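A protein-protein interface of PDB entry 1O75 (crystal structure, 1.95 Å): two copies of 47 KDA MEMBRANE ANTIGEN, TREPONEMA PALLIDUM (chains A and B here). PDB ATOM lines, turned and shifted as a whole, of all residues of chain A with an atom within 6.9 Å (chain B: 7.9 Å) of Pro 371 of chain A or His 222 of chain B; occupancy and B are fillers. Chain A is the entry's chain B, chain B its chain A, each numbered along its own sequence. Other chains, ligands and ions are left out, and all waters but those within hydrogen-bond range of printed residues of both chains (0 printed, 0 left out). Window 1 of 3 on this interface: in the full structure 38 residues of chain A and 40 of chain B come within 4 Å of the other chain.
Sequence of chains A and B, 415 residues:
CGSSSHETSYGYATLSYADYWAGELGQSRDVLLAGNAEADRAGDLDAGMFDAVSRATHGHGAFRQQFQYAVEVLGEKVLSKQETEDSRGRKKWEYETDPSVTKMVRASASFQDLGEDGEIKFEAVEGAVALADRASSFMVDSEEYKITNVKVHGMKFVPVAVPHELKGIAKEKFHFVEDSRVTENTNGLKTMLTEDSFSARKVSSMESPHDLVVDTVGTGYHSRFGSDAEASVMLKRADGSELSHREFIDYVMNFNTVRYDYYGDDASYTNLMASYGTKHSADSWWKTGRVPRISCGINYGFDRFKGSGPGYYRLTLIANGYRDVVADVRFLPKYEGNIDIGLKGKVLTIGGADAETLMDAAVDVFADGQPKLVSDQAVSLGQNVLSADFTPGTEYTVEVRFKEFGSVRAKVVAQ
The backbone carbonyl oxygen of Val 365 of chain A sits at hydrogen-bond distance from the backbone NH of Leu 373 of chain A (2.8 Å).
Of the 19 printed residues of chain B, 3 touch a printed residue of chain A.
Printed residues of chain A that touch a printed residue of chain B: Pro 371 and Leu 373.
Hydrophobic or aromatic side chains of chain A that line the printed part of chain B: Pro 371 and Leu 373.
Among the printed residues, no Asp or Glu carboxylate lies within 4 Å of a Lys or Arg side-chain nitrogen of the other chain.
Among the printed residues, merely in contact across the chains: Pro 371 of chain A with His 222 of chain B (2.9 Å), Pro 371 of chain A with Arg 224 of chain B (3.8 Å), Pro 371 of chain A with Phe 225 of chain B (3.7 Å) and Leu 373 of chain A with Phe 225 of chain B (3.5 Å).
No position is printed for both chains.
Of the 4 pairs that touch across the chains among the printed residues, none has its exchanged pair printed and touching as well.
Of the printed residues of chain B, Leu 373 of chain A touches Phe 225 (3.5 Å).
Of chain A, only Pro 371 (2.9 Å) comes within 4 Å of His 222 of chain B.
Of the printed residues of chain A, Arg 224 of chain B touches Pro 371 (3.8 Å).
Of the printed residues of chain A, Phe 225 of chain B touches Pro 371 and Leu 373.
The nearest residue of chain A that does not touch His 222 of chain B is Gln 370 of chain A (5.2 Å).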
ATOM      1  N   VAL A 365      13.411  22.073  17.166  1.00  0.00           N
ATOM      2  CA  VAL A 365      14.600  22.886  16.965  1.00  0.00           C
ATOM      3  C   VAL A 365      15.751  21.930  16.755  1.00  0.00           C
ATOM      4  O   VAL A 365      15.974  21.034  17.570  1.00  0.00           O
ATOM      5  CB  VAL A 365      14.920  23.781  18.169  1.00  0.00           C
ATOM      6  CG1 VAL A 365      16.184  24.586  17.873  1.00  0.00           C
ATOM      7  CG2 VAL A 365      13.745  24.716  18.459  1.00  0.00           C
ATOM      8  N   PHE A 366      16.473  22.110  15.654  1.00  0.00           N
ATOM      9  CA  PHE A 366      17.586  21.234  15.351  1.00  0.00           C
ATOM     10  C   PHE A 366      18.596  21.895  14.435  1.00  0.00           C
ATOM     11  O   PHE A 366      18.227  22.683  13.562  1.00  0.00           O
ATOM     12  CB  PHE A 366      17.064  19.938  14.711  1.00  0.00           C
ATOM     13  CG  PHE A 366      16.276  20.154  13.444  1.00  0.00           C
ATOM     14  CD1 PHE A 366      16.918  20.230  12.209  1.00  0.00           C
ATOM     15  CD2 PHE A 366      14.891  20.283  13.486  1.00  0.00           C
ATOM     16  CE1 PHE A 366      16.188  20.430  11.030  1.00  0.00           C
ATOM     17  CE2 PHE A 366      14.154  20.483  12.316  1.00  0.00           C
ATOM     18  CZ  PHE A 366      14.804  20.557  11.086  1.00  0.00           C
ATOM     19  N   ALA A 367      19.873  21.587  14.645  1.00  0.00           N
ATOM     20  CA  ALA A 367      20.928  22.140  13.807  1.00  0.00           C
ATOM     21  C   ALA A 367      20.904  21.342  12.509  1.00  0.00           C
ATOM     22  O   ALA A 367      20.652  20.138  12.523  1.00  0.00           O
ATOM     23  CB  ALA A 367      22.270  22.007  14.494  1.00  0.00           C
ATOM     24  N   ASP A 368      21.155  22.027  11.396  1.00  0.00           N
ATOM     25  CA  ASP A 368      21.135  21.436  10.055  1.00  0.00           C
ATOM     26  C   ASP A 368      21.058  19.905   9.978  1.00  0.00           C
ATOM     27  O   ASP A 368      19.975  19.351   9.765  1.00  0.00           O
ATOM     28  CB  ASP A 368      22.327  21.951   9.229  1.00  0.00           C
ATOM     29  CG  ASP A 368      22.326  23.481   9.077  1.00  0.00           C
ATOM     30  OD1 ASP A 368      21.232  24.080   8.941  1.00  0.00           O
ATOM     31  OD2 ASP A 368      23.426  24.087   9.081  1.00  0.00           O
ATOM     32  N   GLY A 369      22.187  19.220  10.151  1.00  0.00           N
ATOM     33  CA  GLY A 369      22.171  17.767  10.074  1.00  0.00           C
ATOM     34  C   GLY A 369      22.426  17.098  11.413  1.00  0.00           C
ATOM     35  O   GLY A 369      23.265  16.195  11.531  1.00  0.00           O
ATOM     36  N   GLN A 370      21.685  17.529  12.426  1.00  0.00           N
ATOM     37  CA  GLN A 370      21.844  16.996  13.768  1.00  0.00           C
ATOM     38  C   GLN A 370      20.524  16.549  14.374  1.00  0.00           C
ATOM     39  O   GLN A 370      19.458  16.860  13.855  1.00  0.00           O
ATOM     40  CB  GLN A 370      22.463  18.068  14.660  1.00  0.00           C
ATOM     41  CG  GLN A 370      23.846  18.501  14.227  1.00  0.00           C
ATOM     42  CD  GLN A 370      24.879  17.419  14.460  1.00  0.00           C
ATOM     43  OE1 GLN A 370      25.031  16.925  15.581  1.00  0.00           O
ATOM     44  NE2 GLN A 370      25.597  17.042  13.408  1.00  0.00           N
ATOM     45  N   PRO A 371      20.581  15.789  15.481  1.00  0.00           N
ATOM     46  CA  PRO A 371      19.357  15.321  16.142  1.00  0.00           C
ATOM     47  C   PRO A 371      18.657  16.534  16.748  1.00  0.00           C
ATOM     48  O   PRO A 371      19.302  17.535  17.027  1.00  0.00           O
ATOM     49  CB  PRO A 371      19.882  14.377  17.222  1.00  0.00           C
ATOM     50  CG  PRO A 371      21.173  13.874  16.640  1.00  0.00           C
ATOM     51  CD  PRO A 371      21.768  15.119  16.041  1.00  0.00           C
ATOM     52  N   LYS A 372      17.349  16.439  16.953  1.00  0.00           N
ATOM     53  CA  LYS A 372      16.575  17.540  17.519  1.00  0.00           C
ATOM     54  C   LYS A 372      16.959  17.837  18.955  1.00  0.00           C
ATOM     55  O   LYS A 372      17.153  16.920  19.756  1.00  0.00           O
ATOM     56  CB  LYS A 372      15.073  17.223  17.476  1.00  0.00           C
ATOM     57  CG  LYS A 372      14.461  17.220  16.086  1.00  0.00           C
ATOM     58  CD  LYS A 372      13.007  16.768  16.129  1.00  0.00           C
ATOM     59  CE  LYS A 372      12.414  16.695  14.723  1.00  0.00           C
ATOM     60  NZ  LYS A 372      11.041  16.098  14.718  1.00  0.00           N
ATOM     61  N   LEU A 373      17.075  19.122  19.279  1.00  0.00           N
ATOM     62  CA  LEU A 373      17.390  19.534  20.643  1.00  0.00           C
ATOM     63  C   LEU A 373      16.056  19.739  21.340  1.00  0.00           C
ATOM     64  O   LEU A 373      15.916  19.515  22.538  1.00  0.00           O
ATOM     65  CB  LEU A 373      18.166  20.851  20.658  1.00  0.00           C
ATOM     66  CG  LEU A 373      19.478  20.958  19.876  1.00  0.00           C
ATOM     67  CD1 LEU A 373      20.200  22.214  20.337  1.00  0.00           C
ATOM     68  CD2 LEU A 373      20.361  19.734  20.114  1.00  0.00           C
ATOM     69  N   VAL A 374      15.072  20.162  20.553  1.00  0.00           N
ATOM     70  CA  VAL A 374      13.724  20.432  21.036  1.00  0.00           C
ATOM     71  C   VAL A 374      12.719  19.688  20.154  1.00  0.00           C
ATOM     72  O   VAL A 374      12.734  19.834  18.933  1.00  0.00           O
ATOM     73  CB  VAL A 374      13.439  21.956  20.970  1.00  0.00           C
ATOM     74  CG1 VAL A 374      12.004  22.247  21.330  1.00  0.00           C
ATOM     75  CG2 VAL A 374      14.391  22.701  21.901  1.00  0.00           C
ATOM     76  N   GLY B 218      25.855   0.540  11.466  1.00  0.00           N
ATOM     77  CA  GLY B 218      26.184   1.855  10.954  1.00  0.00           C
ATOM     78  C   GLY B 218      26.633   2.826  12.020  1.00  0.00           C
ATOM     79  O   GLY B 218      26.410   2.604  13.213  1.00  0.00           O
ATOM     80  N   THR B 219      27.275   3.907  11.589  1.00  0.00           N
ATOM     81  CA  THR B 219      27.741   4.924  12.519  1.00  0.00           C
ATOM     82  C   THR B 219      27.228   6.291  12.084  1.00  0.00           C
ATOM     83  O   THR B 219      27.467   7.280  12.763  1.00  0.00           O
ATOM     84  CB  THR B 219      29.285   4.974  12.591  1.00  0.00           C
ATOM     85  OG1 THR B 219      29.812   5.230  11.286  1.00  0.00           O
ATOM     86  CG2 THR B 219      29.838   3.652  13.079  1.00  0.00           C
ATOM     87  N   GLY B 220      26.495   6.329  10.970  1.00  0.00           N
ATOM     88  CA  GLY B 220      25.972   7.586  10.452  1.00  0.00           C
ATOM     89  C   GLY B 220      24.625   8.073  10.975  1.00  0.00           C
ATOM     90  O   GLY B 220      24.246   9.210  10.719  1.00  0.00           O
ATOM     91  N   TYR B 221      23.882   7.226  11.678  1.00  0.00           N
ATOM     92  CA  TYR B 221      22.591   7.647  12.213  1.00  0.00           C
ATOM     93  C   TYR B 221      22.787   8.189  13.614  1.00  0.00           C
ATOM     94  O   TYR B 221      23.333   7.498  14.470  1.00  0.00           O
ATOM     95  CB  TYR B 221      21.599   6.476  12.319  1.00  0.00           C
ATOM     96  CG  TYR B 221      21.104   5.904  11.015  1.00  0.00           C
ATOM     97  CD1 TYR B 221      20.656   6.740   9.984  1.00  0.00           C
ATOM     98  CD2 TYR B 221      21.017   4.517  10.831  1.00  0.00           C
ATOM     99  CE1 TYR B 221      20.131   6.209   8.798  1.00  0.00           C
ATOM    100  CE2 TYR B 221      20.494   3.978   9.655  1.00  0.00           C
ATOM    101  CZ  TYR B 221      20.053   4.828   8.642  1.00  0.00           C
ATOM    102  OH  TYR B 221      19.541   4.301   7.473  1.00  0.00           O
ATOM    103  N   HIS B 222      22.341   9.419  13.847  1.00  0.00           N
ATOM    104  CA  HIS B 222      22.431  10.026  15.166  1.00  0.00           C
ATOM    105  C   HIS B 222      20.998  10.330  15.591  1.00  0.00           C
ATOM    106  O   HIS B 222      20.469  11.407  15.337  1.00  0.00           O
ATOM    107  CB  HIS B 222      23.292  11.273  15.095  1.00  0.00           C
ATOM    108  CG  HIS B 222      24.720  10.970  14.775  1.00  0.00           C
ATOM    109  ND1 HIS B 222      25.418  11.073  13.619  1.00  0.00           N
ATOM    110  CD2 HIS B 222      25.580  10.404  15.693  1.00  0.00           C
ATOM    111  CE1 HIS B 222      26.674  10.566  13.856  1.00  0.00           C
ATOM    112  NE2 HIS B 222      26.746  10.170  15.116  1.00  0.00           N
ATOM    113  N   SER B 223      20.387   9.342  16.240  1.00  0.00           N
ATOM    114  CA  SER B 223      19.001   9.411  16.669  1.00  0.00           C
ATOM    115  C   SER B 223      18.732  10.254  17.902  1.00  0.00           C
ATOM    116  O   SER B 223      17.615  10.719  18.095  1.00  0.00           O
ATOM    117  CB  SER B 223      18.459   7.991  16.896  1.00  0.00           C
ATOM    118  OG  SER B 223      19.211   7.308  17.889  1.00  0.00           O
ATOM    119  N   ARG B 224      19.747  10.449  18.732  1.00  0.00           N
ATOM    120  CA  ARG B 224      19.583  11.230  19.947  1.00  0.00           C
ATOM    121  C   ARG B 224      20.776  12.120  20.188  1.00  0.00           C
ATOM    122  O   ARG B 224      21.915  11.734  19.921  1.00  0.00           O
ATOM    123  CB  ARG B 224      19.426  10.313  21.159  1.00  0.00           C
ATOM    124  CG  ARG B 224      18.255   9.380  21.093  1.00  0.00           C
ATOM    125  CD  ARG B 224      18.227   8.488  22.316  1.00  0.00           C
ATOM    126  NE  ARG B 224      16.962   7.766  22.407  1.00  0.00           N
ATOM    127  CZ  ARG B 224      16.573   7.075  23.474  1.00  0.00           C
ATOM    128  NH1 ARG B 224      17.361   7.003  24.544  1.00  0.00           N
ATOM    129  NH2 ARG B 224      15.384   6.483  23.476  1.00  0.00           N
ATOM    130  N   PHE B 225      20.508  13.307  20.715  1.00  0.00           N
ATOM    131  CA  PHE B 225      21.555  14.266  21.038  1.00  0.00           C
ATOM    132  C   PHE B 225      22.232  13.811  22.328  1.00  0.00           C
ATOM    133  O   PHE B 225      21.589  13.198  23.182  1.00  0.00           O
ATOM    134  CB  PHE B 225      20.919  15.644  21.252  1.00  0.00           C
ATOM    135  CG  PHE B 225      21.870  16.683  21.759  1.00  0.00           C
ATOM    136  CD1 PHE B 225      22.730  17.345  20.885  1.00  0.00           C
ATOM    137  CD2 PHE B 225      21.903  17.009  23.112  1.00  0.00           C
ATOM    138  CE1 PHE B 225      23.606  18.318  21.352  1.00  0.00           C
ATOM    139  CE2 PHE B 225      22.778  17.983  23.591  1.00  0.00           C
ATOM    140  CZ  PHE B 225      23.629  18.638  22.711  1.00  0.00           C
ATOM    141  N   GLY B 226      23.523  14.099  22.479  1.00  0.00           N
ATOM    142  CA  GLY B 226      24.200  13.718  23.712  1.00  0.00           C
ATOM    143  C   GLY B 226      25.290  12.648  23.647  1.00  0.00           C
ATOM    144  O   GLY B 226      26.026  12.443  24.611  1.00  0.00           O
ATOM    145  N   SER B 227      25.394  11.953  22.526  1.00  0.00           N
ATOM    146  CA  SER B 227      26.411  10.914  22.377  1.00  0.00           C
ATOM    147  C   SER B 227      27.559  11.433  21.544  1.00  0.00           C
ATOM    148  O   SER B 227      27.359  12.283  20.686  1.00  0.00           O
ATOM    149  CB  SER B 227      25.834   9.702  21.650  1.00  0.00           C
ATOM    150  OG  SER B 227      24.942   8.987  22.477  1.00  0.00           O
ATOM    151  N   ASP B 228      28.761  10.918  21.782  1.00  0.00           N
ATOM    152  CA  ASP B 228      29.892  11.313  20.951  1.00  0.00           C
ATOM    153  C   ASP B 228      29.882  10.427  19.711  1.00  0.00           C
ATOM    154  O   ASP B 228      30.324  10.834  18.640  1.00  0.00           O
ATOM    155  CB  ASP B 228      31.204  11.154  21.710  1.00  0.00           C
ATOM    156  CG  ASP B 228      31.356  12.195  22.786  1.00  0.00           C
ATOM    157  OD1 ASP B 228      31.081  13.374  22.474  1.00  0.00           O
ATOM    158  OD2 ASP B 228      31.736  11.854  23.924  1.00  0.00           O
ATOM    159  N   ALA B 229      29.329   9.219  19.853  1.00  0.00           N
ATOM    160  CA  ALA B 229      29.264   8.278  18.736  1.00  0.00           C
ATOM    161  C   ALA B 229      28.078   7.337  18.926  1.00  0.00           C
ATOM    162  O   ALA B 229      27.673   7.048  20.056  1.00  0.00           O
ATOM    163  CB  ALA B 229      30.575   7.480  18.648  1.00  0.00           C
ATOM    164  N   GLU B 230      27.524   6.847  17.830  1.00  0.00           N
ATOM    165  CA  GLU B 230      26.379   5.972  17.946  1.00  0.00           C
ATOM    166  C   GLU B 230      26.465   4.879  16.913  1.00  0.00           C
ATOM    167  O   GLU B 230      26.758   5.150  15.749  1.00  0.00           O
ATOM    168  CB  GLU B 230      25.086   6.785  17.735  1.00  0.00           C
ATOM    169  CG  GLU B 230      23.801   5.977  17.865  1.00  0.00           C
ATOM    170  CD  GLU B 230      22.535   6.823  17.616  1.00  0.00           C
ATOM    171  OE1 GLU B 230      22.513   8.000  18.029  1.00  0.00           O
ATOM    172  OE2 GLU B 230      21.565   6.296  17.021  1.00  0.00           O
ATOM    173  N   ALA B 231      26.198   3.645  17.335  1.00  0.00           N
ATOM    174  CA  ALA B 231      26.223   2.522  16.410  1.00  0.00           C
ATOM    175  C   ALA B 231      24.800   2.039  16.229  1.00  0.00           C
ATOM    176  O   ALA B 231      24.084   1.801  17.202  1.00  0.00           O
ATOM    177  CB  ALA B 231      27.108   1.364  16.963  1.00  0.00           C
ATOM    178  N   SER B 232      24.394   1.886  14.981  1.00  0.00           N
ATOM    179  CA  SER B 232      23.059   1.406  14.674  1.00  0.00           C
ATOM    180  C   SER B 232      23.230  -0.044  14.256  1.00  0.00           C
ATOM    181  O   SER B 232      23.699  -0.332  13.155  1.00  0.00           O
ATOM    182  CB  SER B 232      22.444   2.210  13.511  1.00  0.00           C
ATOM    183  OG  SER B 232      22.298   3.574  13.886  1.00  0.00           O
ATOM    184  N   TRP B 285      19.135   1.785  23.097  1.00  0.00           N
ATOM    185  CA  TRP B 285      17.691   1.930  22.964  1.00  0.00           C
ATOM    186  C   TRP B 285      17.177   1.235  21.722  1.00  0.00           C
ATOM    187  O   TRP B 285      17.932   0.935  20.788  1.00  0.00           O
ATOM    188  CB  TRP B 285      17.297   3.422  22.968  1.00  0.00           C
ATOM    189  CG  TRP B 285      18.007   4.267  21.955  1.00  0.00           C
ATOM    190  CD1 TRP B 285      17.585   4.563  20.681  1.00  0.00           C
ATOM    191  CD2 TRP B 285      19.285   4.901  22.112  1.00  0.00           C
ATOM    192  NE1 TRP B 285      18.527   5.343  20.036  1.00  0.00           N
ATOM    193  CE2 TRP B 285      19.580   5.558  20.892  1.00  0.00           C
ATOM    194  CE3 TRP B 285      20.216   4.970  23.164  1.00  0.00           C
ATOM    195  CZ2 TRP B 285      20.776   6.276  20.696  1.00  0.00           C
ATOM    196  CZ3 TRP B 285      21.402   5.681  22.966  1.00  0.00           C
ATOM    197  CH2 TRP B 285      21.669   6.323  21.738  1.00  0.00           C
ATOM    198  N   SER B 295      20.194   0.574  18.894  1.00  0.00           N
ATOM    199  CA  SER B 295      21.171   1.642  18.874  1.00  0.00           C
ATOM    200  C   SER B 295      21.972   1.607  20.157  1.00  0.00           C
ATOM    201  O   SER B 295      21.430   1.354  21.234  1.00  0.00           O
ATOM    202  CB  SER B 295      20.463   2.996  18.731  1.00  0.00           C
ATOM    203  OG  SER B 295      19.660   3.026  17.563  1.00  0.00           O
ATOM    204  N   PHE B 331      34.715   4.147  15.305  1.00  0.00           N
ATOM    205  CA  PHE B 331      34.276   5.532  15.436  1.00  0.00           C
ATOM    206  C   PHE B 331      35.508   6.396  15.077  1.00  0.00           C
ATOM    207  O   PHE B 331      36.560   6.330  15.725  1.00  0.00           O
ATOM    208  CB  PHE B 331      33.803   5.794  16.869  1.00  0.00           C
ATOM    209  CG  PHE B 331      32.602   4.950  17.280  1.00  0.00           C
ATOM    210  CD1 PHE B 331      31.510   4.791  16.412  1.00  0.00           C
ATOM    211  CD2 PHE B 331      32.548   4.352  18.533  1.00  0.00           C
ATOM    212  CE1 PHE B 331      30.379   4.040  16.798  1.00  0.00           C
ATOM    213  CE2 PHE B 331      31.428   3.604  18.929  1.00  0.00           C
ATOM    214  CZ  PHE B 331      30.342   3.447  18.063  1.00  0.00           C
ATOM    215  N   SER B 407      33.347  13.255   9.071  1.00  0.00           N
ATOM    216  CA  SER B 407      33.074  14.186   7.992  1.00  0.00           C
ATOM    217  C   SER B 407      32.855  15.604   8.498  1.00  0.00           C
ATOM    218  O   SER B 407      32.475  15.813   9.652  1.00  0.00           O
ATOM    219  CB  SER B 407      31.855  13.727   7.200  1.00  0.00           C
ATOM    220  OG  SER B 407      30.695  13.755   8.008  1.00  0.00           O
